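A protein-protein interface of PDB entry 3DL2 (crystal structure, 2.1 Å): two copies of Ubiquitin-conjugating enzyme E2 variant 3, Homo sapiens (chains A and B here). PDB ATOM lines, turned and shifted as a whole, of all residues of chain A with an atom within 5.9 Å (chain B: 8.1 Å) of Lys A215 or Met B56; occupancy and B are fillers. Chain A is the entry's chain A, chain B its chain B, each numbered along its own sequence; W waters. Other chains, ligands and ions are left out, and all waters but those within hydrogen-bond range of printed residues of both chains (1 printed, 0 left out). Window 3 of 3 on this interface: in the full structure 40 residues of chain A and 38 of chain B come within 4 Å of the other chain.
NH2 of Arg A157 is in salt-bridge range of OD2 of Asp B57, at 2.7 Å.
The backbone carbonyl oxygen (O) of Lys B52 lies within hydrogen-bond range of the side-chain amino group (NZ) of Lys A215, 3.2 Å away.
The guanidinium group (NH1) of Arg A157 sits at hydrogen-bond distance from the backbone carbonyl oxygen (O) of Gly A216, at 2.8 Å.
O of Tyr A160 sits at hydrogen-bond distance from N of Val A165 (3.4 Å).
Among the printed residues, merely in contact across the chains: Arg A157 with Ile B60, Tyr A160 with Met B56, Tyr A160 with Ile B60, Lys A215 with Met B56, Trp A220 with Ile B27, Trp A220 with Ala B54 and Trp A220 with Asp B57.
Lys A215 touches just these residues of chain B: Lys B52 (3.2 Å) and Met B56 (3.7 Å).
Of the printed residues of chain A, Met B56 touches Tyr A160 and Lys A215.
No residue of chain B comes within 4 Å of Gly A216.
Of the printed residues of chain A, Ile B60 touches Arg A157 and Tyr A160.
Printed residues of chain B within 4 Å of Arg A157: Asp B57 and Ile B60.
Printed residues of chain A within 4 Å of Lys B52: Lys A215 (3.2 Å).
Of the printed residues of chain B, Trp A220 touches Ile B27, Ala B54 and Asp B57.
Of the printed residues of chain A, Asp B57 touches Arg A157 and Trp A220.
Of the 13 printed residues of chain A, 4 touch a printed residue of chain B.
Among the printed residues, Asp or Glu carboxylates within 4 Å of a Lys or Arg side-chain nitrogen of the other chain: Arg A157 with Asp B57.
No position is printed for both chains.
Water W1 lies within hydrogen-bond range of the side-chain amino group of Lys A215 (2.8 Å), the backbone carbonyl oxygen of Thr B51 (3.1 Å) and the backbone carbonyl oxygen of Lys B52 (3.2 Å).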
ATOM      1  N   ARG A 157      10.900 -16.571  21.235  1.00  0.00           N
ATOM      2  CA  ARG A 157      10.034 -15.516  20.686  1.00  0.00           C
ATOM      3  C   ARG A 157      10.186 -15.350  19.165  1.00  0.00           C
ATOM      4  O   ARG A 157       9.181 -15.297  18.439  1.00  0.00           O
ATOM      5  CB  ARG A 157      10.300 -14.187  21.384  1.00  0.00           C
ATOM      6  CG  ARG A 157       9.826 -14.120  22.832  1.00  0.00           C
ATOM      7  CD  ARG A 157      10.352 -12.859  23.488  1.00  0.00           C
ATOM      8  NE  ARG A 157       9.650 -12.546  24.731  1.00  0.00           N
ATOM      9  CZ  ARG A 157       9.820 -11.419  25.419  1.00  0.00           C
ATOM     10  NH1 ARG A 157      10.701 -10.507  25.005  1.00  0.00           N
ATOM     11  NH2 ARG A 157       9.125 -11.207  26.531  1.00  0.00           N
ATOM     12  N   TYR A 160       8.505 -18.070  17.312  1.00  0.00           N
ATOM     13  CA  TYR A 160       7.056 -17.901  17.407  1.00  0.00           C
ATOM     14  C   TYR A 160       6.572 -16.789  16.480  1.00  0.00           C
ATOM     15  O   TYR A 160       5.525 -16.916  15.849  1.00  0.00           O
ATOM     16  CB  TYR A 160       6.646 -17.594  18.854  1.00  0.00           C
ATOM     17  CG  TYR A 160       5.159 -17.344  19.044  1.00  0.00           C
ATOM     18  CD1 TYR A 160       4.298 -18.379  19.403  1.00  0.00           C
ATOM     19  CD2 TYR A 160       4.617 -16.070  18.861  1.00  0.00           C
ATOM     20  CE1 TYR A 160       2.930 -18.149  19.578  1.00  0.00           C
ATOM     21  CE2 TYR A 160       3.262 -15.834  19.024  1.00  0.00           C
ATOM     22  CZ  TYR A 160       2.426 -16.873  19.386  1.00  0.00           C
ATOM     23  OH  TYR A 160       1.079 -16.630  19.556  1.00  0.00           O
ATOM     24  N   ILE A 161       7.329 -15.693  16.424  1.00  0.00           N
ATOM     25  CA  ILE A 161       7.042 -14.586  15.506  1.00  0.00           C
ATOM     26  C   ILE A 161       6.977 -15.060  14.044  1.00  0.00           C
ATOM     27  O   ILE A 161       6.032 -14.742  13.317  1.00  0.00           O
ATOM     28  CB  ILE A 161       8.063 -13.431  15.675  1.00  0.00           C
ATOM     29  CG1 ILE A 161       7.772 -12.671  16.973  1.00  0.00           C
ATOM     30  CG2 ILE A 161       8.014 -12.475  14.478  1.00  0.00           C
ATOM     31  CD1 ILE A 161       8.952 -11.899  17.536  1.00  0.00           C
ATOM     32  N   VAL A 165       3.072 -15.281  14.163  1.00  0.00           N
ATOM     33  CA  VAL A 165       2.728 -13.887  13.839  1.00  0.00           C
ATOM     34  C   VAL A 165       2.777 -13.645  12.331  1.00  0.00           C
ATOM     35  O   VAL A 165       1.855 -13.055  11.760  1.00  0.00           O
ATOM     36  CB  VAL A 165       3.613 -12.859  14.598  1.00  0.00           C
ATOM     37  CG1 VAL A 165       3.186 -11.428  14.268  1.00  0.00           C
ATOM     38  CG2 VAL A 165       3.529 -13.091  16.101  1.00  0.00           C
ATOM     39  N   GLU A 210      12.874  -7.054  13.922  1.00  0.00           N
ATOM     40  CA  GLU A 210      12.298  -5.775  14.355  1.00  0.00           C
ATOM     41  C   GLU A 210      11.129  -5.998  15.312  1.00  0.00           C
ATOM     42  O   GLU A 210      11.014  -5.311  16.336  1.00  0.00           O
ATOM     43  CB  GLU A 210      11.852  -4.924  13.161  1.00  0.00           C
ATOM     44  CG  GLU A 210      12.981  -4.455  12.258  1.00  0.00           C
ATOM     45  CD  GLU A 210      13.846  -3.340  12.849  1.00  0.00           C
ATOM     46  OE1 GLU A 210      13.694  -2.985  14.039  1.00  0.00           O
ATOM     47  OE2 GLU A 210      14.684  -2.798  12.096  1.00  0.00           O
ATOM     48  N   LEU A 211      10.276  -6.969  14.985  1.00  0.00           N
ATOM     49  CA  LEU A 211       9.143  -7.324  15.849  1.00  0.00           C
ATOM     50  C   LEU A 211       9.607  -7.778  17.234  1.00  0.00           C
ATOM     51  O   LEU A 211       9.011  -7.411  18.252  1.00  0.00           O
ATOM     52  CB  LEU A 211       8.262  -8.393  15.193  1.00  0.00           C
ATOM     53  CG  LEU A 211       7.526  -7.957  13.920  1.00  0.00           C
ATOM     54  CD1 LEU A 211       6.846  -9.143  13.243  1.00  0.00           C
ATOM     55  CD2 LEU A 211       6.521  -6.861  14.233  1.00  0.00           C
ATOM     56  N   LEU A 212      10.674  -8.571  17.257  1.00  0.00           N
ATOM     57  CA  LEU A 212      11.255  -9.053  18.507  1.00  0.00           C
ATOM     58  C   LEU A 212      11.868  -7.934  19.354  1.00  0.00           C
ATOM     59  O   LEU A 212      11.680  -7.906  20.566  1.00  0.00           O
ATOM     60  CB  LEU A 212      12.310 -10.132  18.222  1.00  0.00           C
ATOM     61  CG  LEU A 212      13.149 -10.632  19.403  1.00  0.00           C
ATOM     62  CD1 LEU A 212      12.287 -11.446  20.364  1.00  0.00           C
ATOM     63  CD2 LEU A 212      14.332 -11.451  18.910  1.00  0.00           C
ATOM     64  N   ARG A 213      12.596  -7.026  18.711  1.00  0.00           N
ATOM     65  CA  ARG A 213      13.429  -6.034  19.409  1.00  0.00           C
ATOM     66  C   ARG A 213      12.658  -4.977  20.195  1.00  0.00           C
ATOM     67  O   ARG A 213      13.198  -4.366  21.120  1.00  0.00           O
ATOM     68  CB  ARG A 213      14.380  -5.348  18.429  1.00  0.00           C
ATOM     69  CG  ARG A 213      15.580  -6.195  18.011  1.00  0.00           C
ATOM     70  CD  ARG A 213      16.501  -5.446  17.036  1.00  0.00           C
ATOM     71  NE  ARG A 213      16.980  -4.197  17.625  1.00  0.00           N
ATOM     72  CZ  ARG A 213      16.698  -2.982  17.165  1.00  0.00           C
ATOM     73  NH1 ARG A 213      15.956  -2.829  16.075  1.00  0.00           N
ATOM     74  NH2 ARG A 213      17.178  -1.916  17.793  1.00  0.00           N
ATOM     75  N   VAL A 214      11.403  -4.747  19.826  1.00  0.00           N
ATOM     76  CA  VAL A 214      10.601  -3.741  20.524  1.00  0.00           C
ATOM     77  C   VAL A 214      10.030  -4.287  21.847  1.00  0.00           C
ATOM     78  O   VAL A 214       9.632  -3.515  22.721  1.00  0.00           O
ATOM     79  CB  VAL A 214       9.510  -3.110  19.585  1.00  0.00           C
ATOM     80  CG1 VAL A 214       8.454  -4.139  19.159  1.00  0.00           C
ATOM     81  CG2 VAL A 214       8.872  -1.873  20.221  1.00  0.00           C
ATOM     82  N   LYS A 215      10.032  -5.612  21.997  1.00  0.00           N
ATOM     83  CA  LYS A 215       9.495  -6.268  23.195  1.00  0.00           C
ATOM     84  C   LYS A 215      10.428  -6.165  24.408  1.00  0.00           C
ATOM     85  O   LYS A 215      11.650  -6.317  24.286  1.00  0.00           O
ATOM     86  CB  LYS A 215       9.190  -7.740  22.904  1.00  0.00           C
ATOM     87  CG  LYS A 215       8.226  -7.939  21.749  1.00  0.00           C
ATOM     88  CD  LYS A 215       7.969  -9.403  21.445  1.00  0.00           C
ATOM     89  CE  LYS A 215       6.841  -9.547  20.419  1.00  0.00           C
ATOM     90  NZ  LYS A 215       5.555  -8.924  20.896  1.00  0.00           N
ATOM     91  N   GLY A 216       9.845  -5.913  25.578  1.00  0.00           N
ATOM     92  CA  GLY A 216      10.597  -5.934  26.832  1.00  0.00           C
ATOM     93  C   GLY A 216      10.855  -7.363  27.274  1.00  0.00           C
ATOM     94  O   GLY A 216      10.352  -8.313  26.663  1.00  0.00           O
ATOM     95  N   GLN A 217      11.647  -7.515  28.335  1.00  0.00           N
ATOM     96  CA  GLN A 217      11.903  -8.826  28.934  1.00  0.00           C
ATOM     97  C   GLN A 217      11.669  -8.774  30.440  1.00  0.00           C
ATOM     98  O   GLN A 217      12.605  -8.641  31.230  1.00  0.00           O
ATOM     99  CB  GLN A 217      13.308  -9.340  28.581  1.00  0.00           C
ATOM    100  CG  GLN A 217      13.481  -9.671  27.093  1.00  0.00           C
ATOM    101  CD  GLN A 217      14.827 -10.308  26.761  1.00  0.00           C
ATOM    102  OE1 GLN A 217      15.184 -11.357  27.296  1.00  0.00           O
ATOM    103  NE2 GLN A 217      15.570  -9.676  25.855  1.00  0.00           N
ATOM    104  N   TRP A 220       8.484 -12.221  34.665  1.00  0.00           N
ATOM    105  CA  TRP A 220       7.602 -13.357  34.384  1.00  0.00           C
ATOM    106  C   TRP A 220       7.988 -14.100  33.099  1.00  0.00           C
ATOM    107  O   TRP A 220       8.012 -15.331  33.073  1.00  0.00           O
ATOM    108  CB  TRP A 220       6.113 -12.969  34.424  1.00  0.00           C
ATOM    109  CG  TRP A 220       5.599 -12.105  33.305  1.00  0.00           C
ATOM    110  CD1 TRP A 220       5.484 -10.741  33.308  1.00  0.00           C
ATOM    111  CD2 TRP A 220       5.077 -12.548  32.042  1.00  0.00           C
ATOM    112  NE1 TRP A 220       4.948 -10.307  32.118  1.00  0.00           N
ATOM    113  CE2 TRP A 220       4.688 -11.393  31.323  1.00  0.00           C
ATOM    114  CE3 TRP A 220       4.909 -13.805  31.445  1.00  0.00           C
ATOM    115  CZ2 TRP A 220       4.139 -11.458  30.035  1.00  0.00           C
ATOM    116  CZ3 TRP A 220       4.362 -13.867  30.160  1.00  0.00           C
ATOM    117  CH2 TRP A 220       3.986 -12.701  29.474  1.00  0.00           C
ATOM    118  N   GLY B  22      -4.157  -9.680  30.835  1.00  0.00           N
ATOM    119  CA  GLY B  22      -2.881 -10.358  30.641  1.00  0.00           C
ATOM    120  C   GLY B  22      -1.680  -9.539  31.074  1.00  0.00           C
ATOM    121  O   GLY B  22      -0.574  -9.765  30.584  1.00  0.00           O
ATOM    122  N   ILE B  27      -1.043 -12.520  34.819  1.00  0.00           N
ATOM    123  CA  ILE B  27      -0.035 -13.575  34.696  1.00  0.00           C
ATOM    124  C   ILE B  27       0.237 -14.238  36.050  1.00  0.00           C
ATOM    125  O   ILE B  27       0.305 -15.469  36.143  1.00  0.00           O
ATOM    126  CB  ILE B  27       1.287 -13.013  34.101  1.00  0.00           C
ATOM    127  CG1 ILE B  27       1.063 -12.457  32.685  1.00  0.00           C
ATOM    128  CG2 ILE B  27       2.424 -14.064  34.137  1.00  0.00           C
ATOM    129  CD1 ILE B  27       0.594 -13.484  31.676  1.00  0.00           C
ATOM    130  N   LEU B  44      -7.261 -17.243  29.949  1.00  0.00           N
ATOM    131  CA  LEU B  44      -6.704 -15.919  30.198  1.00  0.00           C
ATOM    132  C   LEU B  44      -7.177 -15.010  29.079  1.00  0.00           C
ATOM    133  O   LEU B  44      -6.848 -15.231  27.908  1.00  0.00           O
ATOM    134  CB  LEU B  44      -5.165 -15.948  30.261  1.00  0.00           C
ATOM    135  CG  LEU B  44      -4.437 -14.608  30.487  1.00  0.00           C
ATOM    136  CD1 LEU B  44      -4.700 -14.058  31.862  1.00  0.00           C
ATOM    137  CD2 LEU B  44      -2.954 -14.764  30.319  1.00  0.00           C
ATOM    138  N   ASP B  46      -6.742 -11.856  27.191  1.00  0.00           N
ATOM    139  CA  ASP B  46      -5.755 -10.829  26.892  1.00  0.00           C
ATOM    140  C   ASP B  46      -6.490  -9.714  26.162  1.00  0.00           C
ATOM    141  O   ASP B  46      -6.830  -9.853  24.981  1.00  0.00           O
ATOM    142  CB  ASP B  46      -4.643 -11.425  26.021  1.00  0.00           C
ATOM    143  CG  ASP B  46      -3.569 -10.409  25.640  1.00  0.00           C
ATOM    144  OD1 ASP B  46      -3.617  -9.253  26.118  1.00  0.00           O
ATOM    145  OD2 ASP B  46      -2.667 -10.779  24.853  1.00  0.00           O
ATOM    146  N   GLY B  50      -3.508  -6.229  20.533  1.00  0.00           N
ATOM    147  CA  GLY B  50      -2.883  -7.501  20.130  1.00  0.00           C
ATOM    148  C   GLY B  50      -1.500  -7.358  19.524  1.00  0.00           C
ATOM    149  O   GLY B  50      -0.731  -8.324  19.462  1.00  0.00           O
ATOM    150  N   THR B  51      -1.199  -6.138  19.082  1.00  0.00           N
ATOM    151  CA  THR B  51       0.106  -5.760  18.551  1.00  0.00           C
ATOM    152  C   THR B  51       1.228  -5.956  19.577  1.00  0.00           C
ATOM    153  O   THR B  51       2.335  -6.378  19.225  1.00  0.00           O
ATOM    154  CB  THR B  51       0.102  -4.287  18.120  1.00  0.00           C
ATOM    155  OG1 THR B  51      -1.230  -3.889  17.767  1.00  0.00           O
ATOM    156  CG2 THR B  51       1.031  -4.074  16.941  1.00  0.00           C
ATOM    157  N   LYS B  52       0.925  -5.652  20.841  1.00  0.00           N
ATOM    158  CA  LYS B  52       1.887  -5.765  21.941  1.00  0.00           C
ATOM    159  C   LYS B  52       2.303  -7.210  22.212  1.00  0.00           C
ATOM    160  O   LYS B  52       3.386  -7.458  22.755  1.00  0.00           O
ATOM    161  CB  LYS B  52       1.324  -5.130  23.219  1.00  0.00           C
ATOM    162  CG  LYS B  52       1.257  -3.606  23.183  1.00  0.00           C
ATOM    163  N   GLY B  53       1.443  -8.155  21.829  1.00  0.00           N
ATOM    164  CA  GLY B  53       1.683  -9.580  22.067  1.00  0.00           C
ATOM    165  C   GLY B  53       1.885  -9.856  23.546  1.00  0.00           C
ATOM    166  O   GLY B  53       2.744 -10.652  23.924  1.00  0.00           O
ATOM    167  N   ALA B  54       1.079  -9.192  24.375  1.00  0.00           N
ATOM    168  CA  ALA B  54       1.250  -9.190  25.832  1.00  0.00           C
ATOM    169  C   ALA B  54       1.504 -10.572  26.444  1.00  0.00           C
ATOM    170  O   ALA B  54       2.313 -10.708  27.362  1.00  0.00           O
ATOM    171  CB  ALA B  54       0.056  -8.520  26.499  1.00  0.00           C
ATOM    172  N   THR B  55       0.835 -11.591  25.912  1.00  0.00           N
ATOM    173  CA  THR B  55       0.877 -12.937  26.485  1.00  0.00           C
ATOM    174  C   THR B  55       1.627 -13.976  25.647  1.00  0.00           C
ATOM    175  O   THR B  55       1.516 -15.176  25.915  1.00  0.00           O
ATOM    176  CB  THR B  55      -0.540 -13.455  26.697  1.00  0.00           C
ATOM    177  OG1 THR B  55      -1.222 -13.450  25.439  1.00  0.00           O
ATOM    178  CG2 THR B  55      -1.287 -12.573  27.698  1.00  0.00           C
ATOM    179  N   MET B  56       2.389 -13.518  24.651  1.00  0.00           N
ATOM    180  CA  MET B  56       3.144 -14.397  23.743  1.00  0.00           C
ATOM    181  C   MET B  56       3.959 -15.472  24.480  1.00  0.00           C
ATOM    182  O   MET B  56       3.972 -16.639  24.077  1.00  0.00           O
ATOM    183  CB  MET B  56       4.076 -13.571  22.840  1.00  0.00           C
ATOM    184  CG  MET B  56       5.079 -14.401  22.035  1.00  0.00           C
ATOM    185  SD  MET B  56       6.181 -13.468  20.936  1.00  0.00           S
ATOM    186  CE  MET B  56       4.985 -12.649  19.872  1.00  0.00           C
ATOM    187  N   ASP B  57       4.632 -15.069  25.556  1.00  0.00           N
ATOM    188  CA  ASP B  57       5.502 -15.982  26.299  1.00  0.00           C
ATOM    189  C   ASP B  57       4.723 -17.120  26.958  1.00  0.00           C
ATOM    190  O   ASP B  57       5.193 -18.262  27.006  1.00  0.00           O
ATOM    191  CB  ASP B  57       6.333 -15.211  27.324  1.00  0.00           C
ATOM    192  CG  ASP B  57       7.219 -14.165  26.675  1.00  0.00           C
ATOM    193  OD1 ASP B  57       7.859 -14.472  25.642  1.00  0.00           O
ATOM    194  OD2 ASP B  57       7.263 -13.033  27.189  1.00  0.00           O
ATOM    195  N   LEU B  58       3.528 -16.804  27.445  1.00  0.00           N
ATOM    196  CA  LEU B  58       2.649 -17.802  28.036  1.00  0.00           C
ATOM    197  C   LEU B  58       2.124 -18.812  26.999  1.00  0.00           C
ATOM    198  O   LEU B  58       1.966 -19.993  27.311  1.00  0.00           O
ATOM    199  CB  LEU B  58       1.505 -17.113  28.782  1.00  0.00           C
ATOM    200  CG  LEU B  58       0.714 -17.924  29.804  1.00  0.00           C
ATOM    201  CD1 LEU B  58       1.591 -18.389  30.967  1.00  0.00           C
ATOM    202  CD2 LEU B  58      -0.437 -17.086  30.309  1.00  0.00           C
ATOM    203  N   GLU B  59       1.866 -18.356  25.774  1.00  0.00           N
ATOM    204  CA  GLU B  59       1.517 -19.256  24.669  1.00  0.00           C
ATOM    205  C   GLU B  59       2.671 -20.210  24.359  1.00  0.00           C
ATOM    206  O   GLU B  59       2.464 -21.414  24.208  1.00  0.00           O
ATOM    207  CB  GLU B  59       1.153 -18.470  23.402  1.00  0.00           C
ATOM    208  CG  GLU B  59      -0.352 -18.274  23.150  1.00  0.00           C
ATOM    209  CD  GLU B  59      -1.106 -19.577  22.844  1.00  0.00           C
ATOM    210  OE1 GLU B  59      -2.117 -19.853  23.533  1.00  0.00           O
ATOM    211  OE2 GLU B  59      -0.696 -20.322  21.921  1.00  0.00           O
ATOM    212  N   ILE B  60       3.878 -19.653  24.262  1.00  0.00           N
ATOM    213  CA  ILE B  60       5.104 -20.412  24.000  1.00  0.00           C
ATOM    214  C   ILE B  60       5.326 -21.479  25.077  1.00  0.00           C
ATOM    215  O   ILE B  60       5.570 -22.648  24.759  1.00  0.00           O
ATOM    216  CB  ILE B  60       6.339 -19.454  23.875  1.00  0.00           C
ATOM    217  CG1 ILE B  60       6.235 -18.615  22.592  1.00  0.00           C
ATOM    218  CG2 ILE B  60       7.666 -20.229  23.904  1.00  0.00           C
ATOM    219  CD1 ILE B  60       7.167 -17.399  22.559  1.00  0.00           C
ATOM    220  N   PHE B  61       5.212 -21.067  26.339  1.00  0.00           N
ATOM    221  CA  PHE B  61       5.334 -21.955  27.503  1.00  0.00           C
ATOM    222  C   PHE B  61       4.334 -23.103  27.474  1.00  0.00           C
ATOM    223  O   PHE B  61       4.645 -24.198  27.921  1.00  0.00           O
ATOM    224  CB  PHE B  61       5.147 -21.162  28.805  1.00  0.00           C
ATOM    225  CG  PHE B  61       5.634 -21.882  30.040  1.00  0.00           C
ATOM    226  CD1 PHE B  61       6.947 -22.355  30.123  1.00  0.00           C
ATOM    227  CD2 PHE B  61       4.792 -22.061  31.133  1.00  0.00           C
ATOM    228  CE1 PHE B  61       7.405 -23.013  31.274  1.00  0.00           C
ATOM    229  CE2 PHE B  61       5.241 -22.717  32.291  1.00  0.00           C
ATOM    230  CZ  PHE B  61       6.549 -23.190  32.358  1.00  0.00           C
ATOM    231  N   ASN B  62       3.130 -22.828  26.971  1.00  0.00           N
ATOM    232  CA  ASN B  62       2.119 -23.855  26.694  1.00  0.00           C
ATOM    233  C   ASN B  62       1.750 -24.711  27.911  1.00  0.00           C
ATOM    234  O   ASN B  62       1.995 -25.924  27.934  1.00  0.00           O
ATOM    235  CB  ASN B  62       2.557 -24.736  25.506  1.00  0.00           C
ATOM    236  CG  ASN B  62       1.400 -25.503  24.874  1.00  0.00           C
ATOM    237  OD1 ASN B  62       0.223 -25.190  25.095  1.00  0.00           O
ATOM    238  ND2 ASN B  62       1.735 -26.515  24.075  1.00  0.00           N
ATOM    239  N   ILE B  68      -5.298 -19.107  26.120  1.00  0.00           N
ATOM    240  CA  ILE B  68      -5.235 -17.650  25.974  1.00  0.00           C
ATOM    241  C   ILE B  68      -6.124 -17.195  24.810  1.00  0.00           C
ATOM    242  O   ILE B  68      -6.092 -17.790  23.730  1.00  0.00           O
ATOM    243  CB  ILE B  68      -3.782 -17.168  25.754  1.00  0.00           C
ATOM    244  CG1 ILE B  68      -2.895 -17.606  26.922  1.00  0.00           C
ATOM    245  CG2 ILE B  68      -3.727 -15.649  25.568  1.00  0.00           C
ATOM    246  CD1 ILE B  68      -1.421 -17.563  26.606  1.00  0.00           C
HETATM  247  O   HOH W   1       5.151  -6.179  20.404  1.00  0.00           O
